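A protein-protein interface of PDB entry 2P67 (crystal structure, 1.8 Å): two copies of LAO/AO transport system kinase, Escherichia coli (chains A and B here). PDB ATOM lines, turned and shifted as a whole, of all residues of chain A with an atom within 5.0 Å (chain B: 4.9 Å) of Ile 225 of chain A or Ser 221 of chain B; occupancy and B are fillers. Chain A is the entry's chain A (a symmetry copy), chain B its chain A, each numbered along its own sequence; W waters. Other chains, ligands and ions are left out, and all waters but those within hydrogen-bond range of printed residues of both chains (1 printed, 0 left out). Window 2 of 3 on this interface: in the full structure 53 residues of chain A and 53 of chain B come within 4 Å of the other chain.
Water W1 bridges O of Ile 225 of chain A and SD of Met 218 of chain B.
Ile 225 of chain A touches just these residues of chain B: Gly 187, Ile 188, Met 218 and Ser 221. Ser 221 of chain B touches just one residue of chain A: Ile 225. Of the printed residues of chain A, Gly 187 of chain B touches Ile 225 (3.2 Å) and Arg 227 (3.0 Å). Printed residues of chain B within 4 Å of Leu 226 of chain A: Ile 188 (3.5 Å). Of the printed residues of chain B, Arg 227 of chain A touches Gly 187 and Ile 188. Of the printed residues of chain A, Ile 188 of chain B touches Ile 225, Leu 226 and Arg 227. The nearest printed residue of chain A that does not touch Ser 221 of chain B is Ser 221 of chain A (6.1 Å).
The backbone carbonyl oxygen (O) of Gly 187 of chain B lies within hydrogen-bond range of the guanidinium group (NE) of Arg 227 of chain A (3.0 Å). N of Ile 188 of chain B sits at hydrogen-bond distance from O of Ile 225 of chain A, 2.8 Å away. The backbone NH (N) of Arg 227 of chain A lies within hydrogen-bond range of the backbone carbonyl oxygen (O) of Ile 188 of chain B (2.8 Å).
The backbone carbonyl oxygen (O) of His 217 of chain B is in hydrogen-bond range of the side-chain hydroxyl (OG) of Ser 221 of chain B, at 3.0 Å.
Ser 221 of chain A touches Ile 225 of chain B, and with the chains exchanged Ile 225 of chain A touches Ser 221 of chain B. 6 positions are printed for both chains. Of the 8 pairs that touch across the chains among the printed residues, 2 have their exchanged pair printed and touching as well.
Of the 8 printed residues of chain A, 4 touch a printed residue of chain B. Hydrophobic or aromatic side chains of chain A that line the printed part of chain B: Ile 225 and Leu 226. Hydrophobic or aromatic side chains of chain B that line the printed part of chain A: Ile 188, Met 218 and Ile 225. Along chain B the printed residues that touch a printed residue of chain A span positions 187 to 225. Among the printed residues, 8 pairs touch across the chains.
Among the printed residues, merely in contact across the chains: Ser 221 of chain A with Ile 225 of chain B (3.6 Å), Ile 225 of chain A with Gly 187 of chain B (3.2 Å), Ile 225 of chain A with Met 218 of chain B (3.9 Å), Ile 225 of chain A with Ser 221 of chain B (3.6 Å) and Leu 226 of chain A with Ile 188 of chain B (3.5 Å).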
ATOM      1  N   GLU A 220      -2.125 -15.479 -12.704  1.00  0.00           N
ATOM      2  CA  GLU A 220      -3.027 -16.619 -12.645  1.00  0.00           C
ATOM      3  C   GLU A 220      -3.629 -16.934 -14.009  1.00  0.00           C
ATOM      4  O   GLU A 220      -3.754 -18.111 -14.375  1.00  0.00           O
ATOM      5  CB  GLU A 220      -4.109 -16.395 -11.581  1.00  0.00           C
ATOM      6  CG  GLU A 220      -4.891 -17.639 -11.223  1.00  0.00           C
ATOM      7  CD  GLU A 220      -5.853 -17.369 -10.083  1.00  0.00           C
ATOM      8  OE1 GLU A 220      -6.754 -16.516 -10.263  1.00  0.00           O
ATOM      9  OE2 GLU A 220      -5.706 -18.021  -9.023  1.00  0.00           O
ATOM     10  N   SER A 221      -3.993 -15.905 -14.784  1.00  0.00           N
ATOM     11  CA  SER A 221      -4.527 -16.147 -16.110  1.00  0.00           C
ATOM     12  C   SER A 221      -3.510 -16.940 -16.927  1.00  0.00           C
ATOM     13  O   SER A 221      -3.860 -17.969 -17.522  1.00  0.00           O
ATOM     14  CB  SER A 221      -4.853 -14.830 -16.840  1.00  0.00           C
ATOM     15  OG  SER A 221      -5.879 -14.102 -16.147  1.00  0.00           O
ATOM     16  N   ALA A 222      -2.256 -16.478 -16.933  1.00  0.00           N
ATOM     17  CA  ALA A 222      -1.197 -17.158 -17.690  1.00  0.00           C
ATOM     18  C   ALA A 222      -1.033 -18.613 -17.198  1.00  0.00           C
ATOM     19  O   ALA A 222      -0.970 -19.548 -17.998  1.00  0.00           O
ATOM     20  CB  ALA A 222       0.123 -16.397 -17.549  1.00  0.00           C
ATOM     21  N   LEU A 223      -0.988 -18.798 -15.891  1.00  0.00           N
ATOM     22  CA  LEU A 223      -0.711 -20.135 -15.328  1.00  0.00           C
ATOM     23  C   LEU A 223      -1.884 -21.120 -15.431  1.00  0.00           C
ATOM     24  O   LEU A 223      -1.687 -22.336 -15.380  1.00  0.00           O
ATOM     25  CB  LEU A 223      -0.188 -20.007 -13.893  1.00  0.00           C
ATOM     26  CG  LEU A 223       1.230 -19.420 -13.777  1.00  0.00           C
ATOM     27  CD1 LEU A 223       1.515 -18.944 -12.328  1.00  0.00           C
ATOM     28  CD2 LEU A 223       2.309 -20.403 -14.285  1.00  0.00           C
ATOM     29  N   HIS A 224      -3.103 -20.595 -15.566  1.00  0.00           N
ATOM     30  CA  HIS A 224      -4.260 -21.436 -15.828  1.00  0.00           C
ATOM     31  C   HIS A 224      -4.371 -21.851 -17.305  1.00  0.00           C
ATOM     32  O   HIS A 224      -4.858 -22.918 -17.588  1.00  0.00           O
ATOM     33  CB  HIS A 224      -5.544 -20.741 -15.332  1.00  0.00           C
ATOM     34  CG  HIS A 224      -5.712 -20.777 -13.836  1.00  0.00           C
ATOM     35  ND1 HIS A 224      -6.866 -20.355 -13.216  1.00  0.00           N
ATOM     36  CD2 HIS A 224      -4.895 -21.221 -12.847  1.00  0.00           C
ATOM     37  CE1 HIS A 224      -6.748 -20.517 -11.907  1.00  0.00           C
ATOM     38  NE2 HIS A 224      -5.562 -21.037 -11.655  1.00  0.00           N
ATOM     39  N   ILE A 225      -3.913 -21.006 -18.230  1.00  0.00           N
ATOM     40  CA  ILE A 225      -4.089 -21.229 -19.690  1.00  0.00           C
ATOM     41  C   ILE A 225      -2.964 -22.080 -20.294  1.00  0.00           C
ATOM     42  O   ILE A 225      -3.209 -22.927 -21.157  1.00  0.00           O
ATOM     43  CB  ILE A 225      -4.191 -19.853 -20.431  1.00  0.00           C
ATOM     44  CG1 ILE A 225      -5.542 -19.191 -20.156  1.00  0.00           C
ATOM     45  CG2 ILE A 225      -3.986 -19.979 -21.910  1.00  0.00           C
ATOM     46  CD1 ILE A 225      -5.559 -17.679 -20.639  1.00  0.00           C
ATOM     47  N   LEU A 226      -1.736 -21.845 -19.832  1.00  0.00           N
ATOM     48  CA  LEU A 226      -0.568 -22.646 -20.270  1.00  0.00           C
ATOM     49  C   LEU A 226      -0.554 -24.068 -19.732  1.00  0.00           C
ATOM     50  O   LEU A 226      -0.958 -24.322 -18.588  1.00  0.00           O
ATOM     51  CB  LEU A 226       0.741 -21.975 -19.864  1.00  0.00           C
ATOM     52  CG  LEU A 226       0.910 -20.543 -20.393  1.00  0.00           C
ATOM     53  CD1 LEU A 226       2.141 -19.813 -19.764  1.00  0.00           C
ATOM     54  CD2 LEU A 226       0.991 -20.602 -21.941  1.00  0.00           C
ATOM     55  N   ARG A 227      -0.050 -24.987 -20.561  1.00  0.00           N
ATOM     56  CA  ARG A 227       0.163 -26.390 -20.133  1.00  0.00           C
ATOM     57  C   ARG A 227       0.953 -26.441 -18.817  1.00  0.00           C
ATOM     58  O   ARG A 227       1.925 -25.699 -18.643  1.00  0.00           O
ATOM     59  CB  ARG A 227       0.941 -27.143 -21.223  1.00  0.00           C
ATOM     60  CG  ARG A 227       0.948 -28.666 -21.030  1.00  0.00           C
ATOM     61  CD  ARG A 227       1.161 -29.352 -22.363  1.00  0.00           C
ATOM     62  NE  ARG A 227       0.075 -29.061 -23.307  1.00  0.00           N
ATOM     63  CZ  ARG A 227      -0.030 -29.609 -24.520  1.00  0.00           C
ATOM     64  NH1 ARG A 227      -1.042 -29.289 -25.316  1.00  0.00           N
ATOM     65  NH2 ARG A 227       0.884 -30.474 -24.943  1.00  0.00           N
ATOM     66  N   GLY B 187      -3.457 -27.504 -21.389  1.00  0.00           N
ATOM     67  CA  GLY B 187      -3.367 -26.102 -21.774  1.00  0.00           C
ATOM     68  C   GLY B 187      -2.456 -25.858 -22.963  1.00  0.00           C
ATOM     69  O   GLY B 187      -1.903 -26.797 -23.559  1.00  0.00           O
ATOM     70  N   ILE B 188      -2.263 -24.581 -23.275  1.00  0.00           N
ATOM     71  CA  ILE B 188      -1.461 -24.160 -24.415  1.00  0.00           C
ATOM     72  C   ILE B 188       0.012 -24.552 -24.226  1.00  0.00           C
ATOM     73  O   ILE B 188       0.603 -24.288 -23.167  1.00  0.00           O
ATOM     74  CB  ILE B 188      -1.547 -22.636 -24.573  1.00  0.00           C
ATOM     75  CG1 ILE B 188      -3.010 -22.211 -24.783  1.00  0.00           C
ATOM     76  CG2 ILE B 188      -0.639 -22.148 -25.719  1.00  0.00           C
ATOM     77  CD1 ILE B 188      -3.204 -20.700 -25.049  1.00  0.00           C
ATOM     78  N   HIS B 217     -10.028 -16.687 -28.478  1.00  0.00           N
ATOM     79  CA  HIS B 217      -9.879 -15.851 -27.275  1.00  0.00           C
ATOM     80  C   HIS B 217      -8.769 -16.349 -26.328  1.00  0.00           C
ATOM     81  O   HIS B 217      -7.990 -15.548 -25.798  1.00  0.00           O
ATOM     82  CB  HIS B 217     -11.210 -15.789 -26.527  1.00  0.00           C
ATOM     83  CG  HIS B 217     -11.215 -14.813 -25.399  1.00  0.00           C
ATOM     84  ND1 HIS B 217     -11.473 -13.470 -25.587  1.00  0.00           N
ATOM     85  CD2 HIS B 217     -10.965 -14.971 -24.079  1.00  0.00           C
ATOM     86  CE1 HIS B 217     -11.403 -12.847 -24.422  1.00  0.00           C
ATOM     87  NE2 HIS B 217     -11.090 -13.734 -23.493  1.00  0.00           N
ATOM     88  N   MET B 218      -8.697 -17.666 -26.146  1.00  0.00           N
ATOM     89  CA  MET B 218      -7.750 -18.294 -25.221  1.00  0.00           C
ATOM     90  C   MET B 218      -6.304 -18.023 -25.669  1.00  0.00           C
ATOM     91  O   MET B 218      -5.478 -17.553 -24.874  1.00  0.00           O
ATOM     92  CB  MET B 218      -8.034 -19.809 -25.121  1.00  0.00           C
ATOM     93  CG  MET B 218      -7.045 -20.548 -24.204  1.00  0.00           C
ATOM     94  SD  MET B 218      -7.293 -22.341 -24.233  1.00  0.00           S
ATOM     95  CE  MET B 218      -6.918 -22.769 -25.905  1.00  0.00           C
ATOM     96  N   TYR B 219      -6.000 -18.303 -26.939  1.00  0.00           N
ATOM     97  CA  TYR B 219      -4.654 -18.019 -27.480  1.00  0.00           C
ATOM     98  C   TYR B 219      -4.312 -16.549 -27.365  1.00  0.00           C
ATOM     99  O   TYR B 219      -3.187 -16.178 -27.009  1.00  0.00           O
ATOM    100  CB  TYR B 219      -4.525 -18.489 -28.941  1.00  0.00           C
ATOM    101  CG  TYR B 219      -4.379 -19.979 -28.999  1.00  0.00           C
ATOM    102  CD1 TYR B 219      -3.136 -20.577 -28.759  1.00  0.00           C
ATOM    103  CD2 TYR B 219      -5.473 -20.802 -29.253  1.00  0.00           C
ATOM    104  CE1 TYR B 219      -2.987 -21.958 -28.775  1.00  0.00           C
ATOM    105  CE2 TYR B 219      -5.324 -22.205 -29.267  1.00  0.00           C
ATOM    106  CZ  TYR B 219      -4.065 -22.753 -29.009  1.00  0.00           C
ATOM    107  OH  TYR B 219      -3.872 -24.110 -29.029  1.00  0.00           O
ATOM    108  N   GLU B 220      -5.297 -15.707 -27.648  1.00  0.00           N
ATOM    109  CA  GLU B 220      -5.084 -14.269 -27.565  1.00  0.00           C
ATOM    110  C   GLU B 220      -4.786 -13.825 -26.139  1.00  0.00           C
ATOM    111  O   GLU B 220      -3.917 -12.967 -25.926  1.00  0.00           O
ATOM    112  CB  GLU B 220      -6.280 -13.513 -28.160  1.00  0.00           C
ATOM    113  CG  GLU B 220      -6.019 -12.045 -28.411  1.00  0.00           C
ATOM    114  CD  GLU B 220      -7.195 -11.394 -29.111  1.00  0.00           C
ATOM    115  OE1 GLU B 220      -8.300 -11.384 -28.519  1.00  0.00           O
ATOM    116  OE2 GLU B 220      -7.001 -10.889 -30.242  1.00  0.00           O
ATOM    117  N   SER B 221      -5.477 -14.399 -25.147  1.00  0.00           N
ATOM    118  CA  SER B 221      -5.198 -14.047 -23.768  1.00  0.00           C
ATOM    119  C   SER B 221      -3.729 -14.324 -23.462  1.00  0.00           C
ATOM    120  O   SER B 221      -3.028 -13.446 -22.940  1.00  0.00           O
ATOM    121  CB  SER B 221      -6.083 -14.843 -22.789  1.00  0.00           C
ATOM    122  OG  SER B 221      -7.471 -14.532 -22.986  1.00  0.00           O
ATOM    123  N   ALA B 222      -3.261 -15.527 -23.810  1.00  0.00           N
ATOM    124  CA  ALA B 222      -1.865 -15.904 -23.559  1.00  0.00           C
ATOM    125  C   ALA B 222      -0.906 -14.932 -24.281  1.00  0.00           C
ATOM    126  O   ALA B 222       0.058 -14.439 -23.693  1.00  0.00           O
ATOM    127  CB  ALA B 222      -1.615 -17.341 -24.022  1.00  0.00           C
ATOM    128  N   LEU B 223      -1.186 -14.646 -25.540  1.00  0.00           N
ATOM    129  CA  LEU B 223      -0.263 -13.826 -26.350  1.00  0.00           C
ATOM    130  C   LEU B 223      -0.276 -12.330 -26.003  1.00  0.00           C
ATOM    131  O   LEU B 223       0.684 -11.612 -26.293  1.00  0.00           O
ATOM    132  CB  LEU B 223      -0.504 -14.075 -27.844  1.00  0.00           C
ATOM    133  CG  LEU B 223      -0.062 -15.462 -28.341  1.00  0.00           C
ATOM    134  CD1 LEU B 223      -0.703 -15.785 -29.718  1.00  0.00           C
ATOM    135  CD2 LEU B 223       1.476 -15.605 -28.372  1.00  0.00           C
ATOM    136  N   HIS B 224      -1.365 -11.862 -25.393  1.00  0.00           N
ATOM    137  CA  HIS B 224      -1.416 -10.501 -24.883  1.00  0.00           C
ATOM    138  C   HIS B 224      -0.700 -10.346 -23.531  1.00  0.00           C
ATOM    139  O   HIS B 224      -0.163  -9.300 -23.257  1.00  0.00           O
ATOM    140  CB  HIS B 224      -2.878 -10.014 -24.814  1.00  0.00           C
ATOM    141  CG  HIS B 224      -3.459  -9.655 -26.156  1.00  0.00           C
ATOM    142  ND1 HIS B 224      -4.689  -9.051 -26.286  1.00  0.00           N
ATOM    143  CD2 HIS B 224      -2.965  -9.776 -27.415  1.00  0.00           C
ATOM    144  CE1 HIS B 224      -4.941  -8.832 -27.567  1.00  0.00           C
ATOM    145  NE2 HIS B 224      -3.914  -9.265 -28.274  1.00  0.00           N
ATOM    146  N   ILE B 225      -0.694 -11.391 -22.700  1.00  0.00           N
ATOM    147  CA  ILE B 225      -0.159 -11.322 -21.315  1.00  0.00           C
ATOM    148  C   ILE B 225       1.348 -11.604 -21.252  1.00  0.00           C
ATOM    149  O   ILE B 225       2.077 -10.965 -20.489  1.00  0.00           O
ATOM    150  CB  ILE B 225      -0.940 -12.318 -20.393  1.00  0.00           C
ATOM    151  CG1 ILE B 225      -2.347 -11.794 -20.100  1.00  0.00           C
ATOM    152  CG2 ILE B 225      -0.227 -12.587 -19.102  1.00  0.00           C
ATOM    153  CD1 ILE B 225      -3.256 -12.907 -19.426  1.00  0.00           C
HETATM  154  O   HOH W   1      -5.694 -23.735 -21.385  1.00  0.00           O
